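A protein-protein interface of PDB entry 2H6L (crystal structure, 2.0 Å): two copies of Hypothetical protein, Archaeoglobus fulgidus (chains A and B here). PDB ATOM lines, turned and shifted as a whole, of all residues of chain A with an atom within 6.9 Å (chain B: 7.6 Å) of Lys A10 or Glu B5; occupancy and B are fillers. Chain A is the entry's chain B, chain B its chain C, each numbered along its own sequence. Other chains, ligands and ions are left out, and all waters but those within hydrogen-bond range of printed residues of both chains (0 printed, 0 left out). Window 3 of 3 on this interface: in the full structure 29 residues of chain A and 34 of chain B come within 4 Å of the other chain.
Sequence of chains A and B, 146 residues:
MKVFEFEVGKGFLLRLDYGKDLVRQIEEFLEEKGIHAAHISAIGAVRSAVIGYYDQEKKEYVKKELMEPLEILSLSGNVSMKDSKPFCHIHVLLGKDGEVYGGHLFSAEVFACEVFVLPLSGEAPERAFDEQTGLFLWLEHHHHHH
Val A8 touches its own counterpart, Val B8.
Among the printed residues, merely in contact across the chains: Val A8 with Val B8, Gly A9 with Glu B7, Lys A10 with Glu B5, Lys A10 with Phe B6, Gly A11 with Phe B4, Gly A11 with Glu B5, Phe A12 with Phe B4, Phe A12 with Glu B5, Leu A13 with Val B3, Leu A13 with Phe B6, Leu A13 with Leu B120, Phe A116 with Leu B118 and Phe A116 with Leu B120.
N of Val A117 is in hydrogen-bond range of O of Phe A12, 2.8 Å away. The backbone NH of Glu B7 is in hydrogen-bond range of the backbone carbonyl oxygen of Ser B121.
The backbone carbonyl oxygen (O) of Gly A9 sits at hydrogen-bond distance from the backbone NH (N) of Val B8 (2.8 Å). O of Gly A11 is in hydrogen-bond range of N of Phe B6, at 2.7 Å. The backbone carbonyl oxygen of Leu A13 lies within hydrogen-bond range of the backbone NH of Phe B4 (3.0 Å).
Lys A10 touches two residues of chain B. Glu B5 touches just these residues of chain A: Lys A10 (3.8 Å), Gly A11 (3.5 Å) and Phe A12 (3.3 Å). Of chain B, only Glu B7 and Val B8 come within 4 Å of Gly A9. Of the printed residues of chain B, Phe A116 touches Leu B118 (3.5 Å) and Leu B120 (3.9 Å). Printed residues of chain A within 4 Å of Phe B4: Gly A11, Phe A12 and Leu A13. Printed residues of chain A within 4 Å of Val B8: Val A8 (3.7 Å) and Gly A9 (2.8 Å). Pro A119 touches none of the printed residues of chain B. The nearest residue of chain A that does not touch Glu B5 is Lys A33 (4.8 Å). The nearest printed residue of chain A that does not touch Val B8 is Leu A118 (4.1 Å).
Hydrophobic or aromatic side chains of chain B within 4 Å of the printed part of chain A: Phe B4, Phe B6, Val B8, Leu B118 and Leu B120. Among the printed residues, 16 pairs touch across the chains.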
ATOM      1  N   GLU A   7      23.280  16.403  -1.294  1.00  0.00           N
ATOM      2  CA  GLU A   7      23.054  15.155  -2.005  1.00  0.00           C
ATOM      3  C   GLU A   7      22.241  14.324  -1.028  1.00  0.00           C
ATOM      4  O   GLU A   7      22.477  14.385   0.178  1.00  0.00           O
ATOM      5  CB  GLU A   7      24.368  14.431  -2.294  1.00  0.00           C
ATOM      6  CG  GLU A   7      24.889  14.572  -3.717  1.00  0.00           C
ATOM      7  CD  GLU A   7      26.149  13.748  -3.952  1.00  0.00           C
ATOM      8  OE1 GLU A   7      27.190  14.044  -3.322  1.00  0.00           O
ATOM      9  OE2 GLU A   7      26.093  12.802  -4.769  1.00  0.00           O
ATOM     10  N   VAL A   8      21.273  13.572  -1.539  1.00  0.00           N
ATOM     11  CA  VAL A   8      20.467  12.712  -0.686  1.00  0.00           C
ATOM     12  C   VAL A   8      20.934  11.277  -0.906  1.00  0.00           C
ATOM     13  O   VAL A   8      21.462  10.945  -1.966  1.00  0.00           O
ATOM     14  CB  VAL A   8      18.958  12.821  -1.018  1.00  0.00           C
ATOM     15  CG1 VAL A   8      18.483  14.251  -0.797  1.00  0.00           C
ATOM     16  CG2 VAL A   8      18.700  12.378  -2.447  1.00  0.00           C
ATOM     17  N   GLY A   9      20.747  10.430   0.097  1.00  0.00           N
ATOM     18  CA  GLY A   9      21.170   9.048  -0.025  1.00  0.00           C
ATOM     19  C   GLY A   9      20.376   8.121   0.875  1.00  0.00           C
ATOM     20  O   GLY A   9      19.760   7.165   0.400  1.00  0.00           O
ATOM     21  N   LYS A  10      20.385   8.411   2.173  1.00  0.00           N
ATOM     22  CA  LYS A  10      19.671   7.599   3.149  1.00  0.00           C
ATOM     23  C   LYS A  10      18.317   8.191   3.509  1.00  0.00           C
ATOM     24  O   LYS A  10      18.012   9.336   3.187  1.00  0.00           O
ATOM     25  CB  LYS A  10      20.494   7.455   4.432  1.00  0.00           C
ATOM     26  CG  LYS A  10      21.900   6.919   4.225  1.00  0.00           C
ATOM     27  CD  LYS A  10      22.637   6.789   5.551  1.00  0.00           C
ATOM     28  CE  LYS A  10      24.090   6.399   5.339  1.00  0.00           C
ATOM     29  NZ  LYS A  10      24.205   5.198   4.472  1.00  0.00           N
ATOM     30  N   GLY A  11      17.511   7.387   4.191  1.00  0.00           N
ATOM     31  CA  GLY A  11      16.197   7.814   4.619  1.00  0.00           C
ATOM     32  C   GLY A  11      15.904   7.097   5.920  1.00  0.00           C
ATOM     33  O   GLY A  11      16.348   5.973   6.117  1.00  0.00           O
ATOM     34  N   PHE A  12      15.157   7.740   6.807  1.00  0.00           N
ATOM     35  CA  PHE A  12      14.835   7.138   8.095  1.00  0.00           C
ATOM     36  C   PHE A  12      13.377   7.325   8.489  1.00  0.00           C
ATOM     37  O   PHE A  12      12.790   8.387   8.273  1.00  0.00           O
ATOM     38  CB  PHE A  12      15.691   7.759   9.198  1.00  0.00           C
ATOM     39  CG  PHE A  12      17.157   7.458   9.087  1.00  0.00           C
ATOM     40  CD1 PHE A  12      17.661   6.235   9.513  1.00  0.00           C
ATOM     41  CD2 PHE A  12      18.038   8.407   8.582  1.00  0.00           C
ATOM     42  CE1 PHE A  12      19.022   5.959   9.445  1.00  0.00           C
ATOM     43  CE2 PHE A  12      19.406   8.147   8.505  1.00  0.00           C
ATOM     44  CZ  PHE A  12      19.900   6.919   8.938  1.00  0.00           C
ATOM     45  N   LEU A  13      12.791   6.279   9.055  1.00  0.00           N
ATOM     46  CA  LEU A  13      11.429   6.363   9.552  1.00  0.00           C
ATOM     47  C   LEU A  13      11.583   6.028  11.029  1.00  0.00           C
ATOM     48  O   LEU A  13      12.174   5.016  11.382  1.00  0.00           O
ATOM     49  CB  LEU A  13      10.512   5.352   8.861  1.00  0.00           C
ATOM     50  CG  LEU A  13      10.026   5.694   7.449  1.00  0.00           C
ATOM     51  CD1 LEU A  13       9.164   4.549   6.924  1.00  0.00           C
ATOM     52  CD2 LEU A  13       9.220   6.989   7.464  1.00  0.00           C
ATOM     53  N   LYS A  33      23.305   9.865  15.080  1.00  0.00           N
ATOM     54  CA  LYS A  33      23.692   9.594  13.695  1.00  0.00           C
ATOM     55  C   LYS A  33      24.638  10.639  13.112  1.00  0.00           C
ATOM     56  O   LYS A  33      25.242  10.418  12.065  1.00  0.00           O
ATOM     57  CB  LYS A  33      22.452   9.502  12.795  1.00  0.00           C
ATOM     58  CG  LYS A  33      21.488   8.392  13.170  1.00  0.00           C
ATOM     59  CD  LYS A  33      22.131   7.010  13.038  1.00  0.00           C
ATOM     60  CE  LYS A  33      21.211   5.915  13.573  1.00  0.00           C
ATOM     61  NZ  LYS A  33      21.825   4.556  13.493  1.00  0.00           N
ATOM     62  N   ILE A  35      23.714  13.736  12.115  1.00  0.00           N
ATOM     63  CA  ILE A  35      23.017  14.427  11.027  1.00  0.00           C
ATOM     64  C   ILE A  35      23.006  15.915  11.348  1.00  0.00           C
ATOM     65  O   ILE A  35      22.405  16.320  12.337  1.00  0.00           O
ATOM     66  CB  ILE A  35      21.535  13.997  10.900  1.00  0.00           C
ATOM     67  CG1 ILE A  35      21.409  12.472  10.896  1.00  0.00           C
ATOM     68  CG2 ILE A  35      20.940  14.596   9.623  1.00  0.00           C
ATOM     69  CD1 ILE A  35      22.030  11.815   9.713  1.00  0.00           C
ATOM     70  N   PHE A 116       9.630  11.049   9.450  1.00  0.00           N
ATOM     71  CA  PHE A 116      10.428  10.748   8.269  1.00  0.00           C
ATOM     72  C   PHE A 116      11.603  11.706   8.310  1.00  0.00           C
ATOM     73  O   PHE A 116      11.421  12.919   8.421  1.00  0.00           O
ATOM     74  CB  PHE A 116       9.654  10.979   6.966  1.00  0.00           C
ATOM     75  CG  PHE A 116      10.515  10.852   5.726  1.00  0.00           C
ATOM     76  CD1 PHE A 116      11.335   9.738   5.543  1.00  0.00           C
ATOM     77  CD2 PHE A 116      10.513  11.848   4.748  1.00  0.00           C
ATOM     78  CE1 PHE A 116      12.142   9.615   4.414  1.00  0.00           C
ATOM     79  CE2 PHE A 116      11.312  11.737   3.616  1.00  0.00           C
ATOM     80  CZ  PHE A 116      12.131  10.617   3.444  1.00  0.00           C
ATOM     81  N   VAL A 117      12.809  11.171   8.237  1.00  0.00           N
ATOM     82  CA  VAL A 117      13.979  12.024   8.258  1.00  0.00           C
ATOM     83  C   VAL A 117      14.799  11.812   7.001  1.00  0.00           C
ATOM     84  O   VAL A 117      15.218  10.697   6.696  1.00  0.00           O
ATOM     85  CB  VAL A 117      14.850  11.744   9.491  1.00  0.00           C
ATOM     86  CG1 VAL A 117      16.019  12.712   9.523  1.00  0.00           C
ATOM     87  CG2 VAL A 117      14.013  11.874  10.754  1.00  0.00           C
ATOM     88  N   LEU A 118      15.013  12.893   6.264  1.00  0.00           N
ATOM     89  CA  LEU A 118      15.791  12.840   5.037  1.00  0.00           C
ATOM     90  C   LEU A 118      17.054  13.643   5.289  1.00  0.00           C
ATOM     91  O   LEU A 118      17.044  14.873   5.190  1.00  0.00           O
ATOM     92  CB  LEU A 118      15.001  13.460   3.881  1.00  0.00           C
ATOM     93  CG  LEU A 118      15.605  13.363   2.478  1.00  0.00           C
ATOM     94  CD1 LEU A 118      15.612  11.920   2.022  1.00  0.00           C
ATOM     95  CD2 LEU A 118      14.787  14.195   1.513  1.00  0.00           C
ATOM     96  N   PRO A 119      18.154  12.964   5.657  1.00  0.00           N
ATOM     97  CA  PRO A 119      19.403  13.685   5.909  1.00  0.00           C
ATOM     98  C   PRO A 119      19.950  14.282   4.617  1.00  0.00           C
ATOM     99  O   PRO A 119      19.772  13.720   3.534  1.00  0.00           O
ATOM    100  CB  PRO A 119      20.312  12.604   6.491  1.00  0.00           C
ATOM    101  CG  PRO A 119      19.825  11.358   5.816  1.00  0.00           C
ATOM    102  CD  PRO A 119      18.324  11.518   5.893  1.00  0.00           C
ATOM    103  N   LEU A 120      20.606  15.429   4.733  1.00  0.00           N
ATOM    104  CA  LEU A 120      21.171  16.094   3.569  1.00  0.00           C
ATOM    105  C   LEU A 120      22.682  16.185   3.722  1.00  0.00           C
ATOM    106  O   LEU A 120      23.189  16.811   4.656  1.00  0.00           O
ATOM    107  CB  LEU A 120      20.560  17.490   3.418  1.00  0.00           C
ATOM    108  CG  LEU A 120      19.042  17.487   3.211  1.00  0.00           C
ATOM    109  CD1 LEU A 120      18.497  18.905   3.273  1.00  0.00           C
ATOM    110  CD2 LEU A 120      18.719  16.843   1.877  1.00  0.00           C
ATOM    111  N   LYS B   2      12.211   3.292  17.993  1.00  0.00           N
ATOM    112  CA  LYS B   2      12.420   2.372  16.879  1.00  0.00           C
ATOM    113  C   LYS B   2      12.973   3.133  15.676  1.00  0.00           C
ATOM    114  O   LYS B   2      12.442   4.169  15.287  1.00  0.00           O
ATOM    115  CB  LYS B   2      11.105   1.694  16.497  1.00  0.00           C
ATOM    116  CG  LYS B   2      10.439   0.930  17.626  1.00  0.00           C
ATOM    117  CD  LYS B   2      11.278  -0.255  18.069  1.00  0.00           C
ATOM    118  CE  LYS B   2      10.512  -1.115  19.064  1.00  0.00           C
ATOM    119  NZ  LYS B   2       9.213  -1.559  18.488  1.00  0.00           N
ATOM    120  N   VAL B   3      14.035   2.602  15.083  1.00  0.00           N
ATOM    121  CA  VAL B   3      14.674   3.245  13.946  1.00  0.00           C
ATOM    122  C   VAL B   3      14.719   2.348  12.720  1.00  0.00           C
ATOM    123  O   VAL B   3      15.211   1.226  12.786  1.00  0.00           O
ATOM    124  CB  VAL B   3      16.121   3.645  14.298  1.00  0.00           C
ATOM    125  CG1 VAL B   3      16.806   4.258  13.090  1.00  0.00           C
ATOM    126  CG2 VAL B   3      16.117   4.616  15.472  1.00  0.00           C
ATOM    127  N   PHE B   4      14.205   2.849  11.600  1.00  0.00           N
ATOM    128  CA  PHE B   4      14.218   2.095  10.347  1.00  0.00           C
ATOM    129  C   PHE B   4      15.048   2.863   9.334  1.00  0.00           C
ATOM    130  O   PHE B   4      14.724   3.998   8.993  1.00  0.00           O
ATOM    131  CB  PHE B   4      12.797   1.908   9.817  1.00  0.00           C
ATOM    132  CG  PHE B   4      11.898   1.187  10.770  1.00  0.00           C
ATOM    133  CD1 PHE B   4      11.183   1.881  11.730  1.00  0.00           C
ATOM    134  CD2 PHE B   4      11.799  -0.197  10.736  1.00  0.00           C
ATOM    135  CE1 PHE B   4      10.380   1.203  12.649  1.00  0.00           C
ATOM    136  CE2 PHE B   4      11.005  -0.880  11.645  1.00  0.00           C
ATOM    137  CZ  PHE B   4      10.295  -0.183  12.599  1.00  0.00           C
ATOM    138  N   GLU B   5      16.117   2.236   8.860  1.00  0.00           N
ATOM    139  CA  GLU B   5      17.018   2.866   7.908  1.00  0.00           C
ATOM    140  C   GLU B   5      16.724   2.467   6.470  1.00  0.00           C
ATOM    141  O   GLU B   5      16.369   1.315   6.196  1.00  0.00           O
ATOM    142  CB  GLU B   5      18.465   2.516   8.250  1.00  0.00           C
ATOM    143  CG  GLU B   5      19.506   3.308   7.473  1.00  0.00           C
ATOM    144  CD  GLU B   5      20.897   3.134   8.041  1.00  0.00           C
ATOM    145  OE1 GLU B   5      21.013   2.602   9.164  1.00  0.00           O
ATOM    146  OE2 GLU B   5      21.870   3.535   7.372  1.00  0.00           O
ATOM    147  N   PHE B   6      16.879   3.429   5.559  1.00  0.00           N
ATOM    148  CA  PHE B   6      16.622   3.204   4.137  1.00  0.00           C
ATOM    149  C   PHE B   6      17.563   4.001   3.229  1.00  0.00           C
ATOM    150  O   PHE B   6      18.381   4.801   3.688  1.00  0.00           O
ATOM    151  CB  PHE B   6      15.197   3.620   3.769  1.00  0.00           C
ATOM    152  CG  PHE B   6      14.123   3.009   4.627  1.00  0.00           C
ATOM    153  CD1 PHE B   6      13.730   3.619   5.813  1.00  0.00           C
ATOM    154  CD2 PHE B   6      13.480   1.841   4.227  1.00  0.00           C
ATOM    155  CE1 PHE B   6      12.706   3.076   6.590  1.00  0.00           C
ATOM    156  CE2 PHE B   6      12.456   1.286   4.996  1.00  0.00           C
ATOM    157  CZ  PHE B   6      12.066   1.905   6.180  1.00  0.00           C
ATOM    158  N   GLU B   7      17.429   3.763   1.929  1.00  0.00           N
ATOM    159  CA  GLU B   7      18.188   4.475   0.904  1.00  0.00           C
ATOM    160  C   GLU B   7      17.121   5.012  -0.045  1.00  0.00           C
ATOM    161  O   GLU B   7      16.077   4.383  -0.228  1.00  0.00           O
ATOM    162  CB  GLU B   7      19.110   3.529   0.128  1.00  0.00           C
ATOM    163  CG  GLU B   7      20.564   3.515   0.582  1.00  0.00           C
ATOM    164  CD  GLU B   7      21.432   2.619  -0.286  1.00  0.00           C
ATOM    165  OE1 GLU B   7      21.299   1.373  -0.203  1.00  0.00           O
ATOM    166  OE2 GLU B   7      22.247   3.165  -1.062  1.00  0.00           O
ATOM    167  N   VAL B   8      17.363   6.182  -0.624  1.00  0.00           N
ATOM    168  CA  VAL B   8      16.418   6.761  -1.568  1.00  0.00           C
ATOM    169  C   VAL B   8      17.040   6.685  -2.960  1.00  0.00           C
ATOM    170  O   VAL B   8      18.260   6.727  -3.101  1.00  0.00           O
ATOM    171  CB  VAL B   8      16.110   8.229  -1.225  1.00  0.00           C
ATOM    172  CG1 VAL B   8      15.492   8.312   0.163  1.00  0.00           C
ATOM    173  CG2 VAL B   8      17.381   9.061  -1.298  1.00  0.00           C
ATOM    174  N   LEU B 118       7.942   8.960  -2.436  1.00  0.00           N
ATOM    175  CA  LEU B 118       9.372   8.734  -2.296  1.00  0.00           C
ATOM    176  C   LEU B 118       9.550   7.340  -1.708  1.00  0.00           C
ATOM    177  O   LEU B 118       9.443   7.152  -0.493  1.00  0.00           O
ATOM    178  CB  LEU B 118       9.975   9.787  -1.359  1.00  0.00           C
ATOM    179  CG  LEU B 118      11.488   9.806  -1.143  1.00  0.00           C
ATOM    180  CD1 LEU B 118      12.194  10.145  -2.438  1.00  0.00           C
ATOM    181  CD2 LEU B 118      11.832  10.838  -0.081  1.00  0.00           C
ATOM    182  N   LEU B 120      11.169   4.025  -0.201  1.00  0.00           N
ATOM    183  CA  LEU B 120      12.293   3.852   0.703  1.00  0.00           C
ATOM    184  C   LEU B 120      12.764   2.406   0.608  1.00  0.00           C
ATOM    185  O   LEU B 120      12.032   1.472   0.944  1.00  0.00           O
ATOM    186  CB  LEU B 120      11.863   4.207   2.136  1.00  0.00           C
ATOM    187  CG  LEU B 120      11.486   5.683   2.322  1.00  0.00           C
ATOM    188  CD1 LEU B 120      10.803   5.924   3.662  1.00  0.00           C
ATOM    189  CD2 LEU B 120      12.742   6.522   2.201  1.00  0.00           C
ATOM    190  N   SER B 121      13.984   2.235   0.121  1.00  0.00           N
ATOM    191  CA  SER B 121      14.589   0.922  -0.042  1.00  0.00           C
ATOM    192  C   SER B 121      15.249   0.454   1.260  1.00  0.00           C
ATOM    193  O   SER B 121      16.271   0.997   1.685  1.00  0.00           O
ATOM    194  CB  SER B 121      15.630   0.982  -1.163  1.00  0.00           C
ATOM    195  OG  SER B 121      16.271  -0.265  -1.342  1.00  0.00           O
ATOM    196  N   GLY B 122      14.658  -0.559   1.883  1.00  0.00           N
ATOM    197  CA  GLY B 122      15.186  -1.089   3.127  1.00  0.00           C
ATOM    198  C   GLY B 122      14.123  -1.953   3.766  1.00  0.00           C
ATOM    199  O   GLY B 122      13.099  -2.245   3.140  1.00  0.00           O
ATOM    200  N   GLU B 123      14.346  -2.371   5.006  1.00  0.00           N
ATOM    201  CA  GLU B 123      13.355  -3.204   5.674  1.00  0.00           C
ATOM    202  C   GLU B 123      12.108  -2.385   5.955  1.00  0.00           C
ATOM    203  O   GLU B 123      12.153  -1.391   6.673  1.00  0.00           O
ATOM    204  CB  GLU B 123      13.917  -3.772   6.976  1.00  0.00           C
ATOM    205  CG  GLU B 123      15.098  -4.701   6.763  1.00  0.00           C
ATOM    206  CD  GLU B 123      14.777  -5.831   5.798  1.00  0.00           C
ATOM    207  OE1 GLU B 123      13.672  -6.404   5.910  1.00  0.00           O
ATOM    208  OE2 GLU B 123      15.630  -6.157   4.942  1.00  0.00           O
ATOM    209  N   ALA B 124      10.995  -2.801   5.361  1.00  0.00           N
ATOM    210  CA  ALA B 124       9.726  -2.115   5.552  1.00  0.00           C
ATOM    211  C   ALA B 124       9.191  -2.386   6.955  1.00  0.00           C
ATOM    212  O   ALA B 124       9.135  -3.536   7.399  1.00  0.00           O
ATOM    213  CB  ALA B 124       8.718  -2.590   4.509  1.00  0.00           C
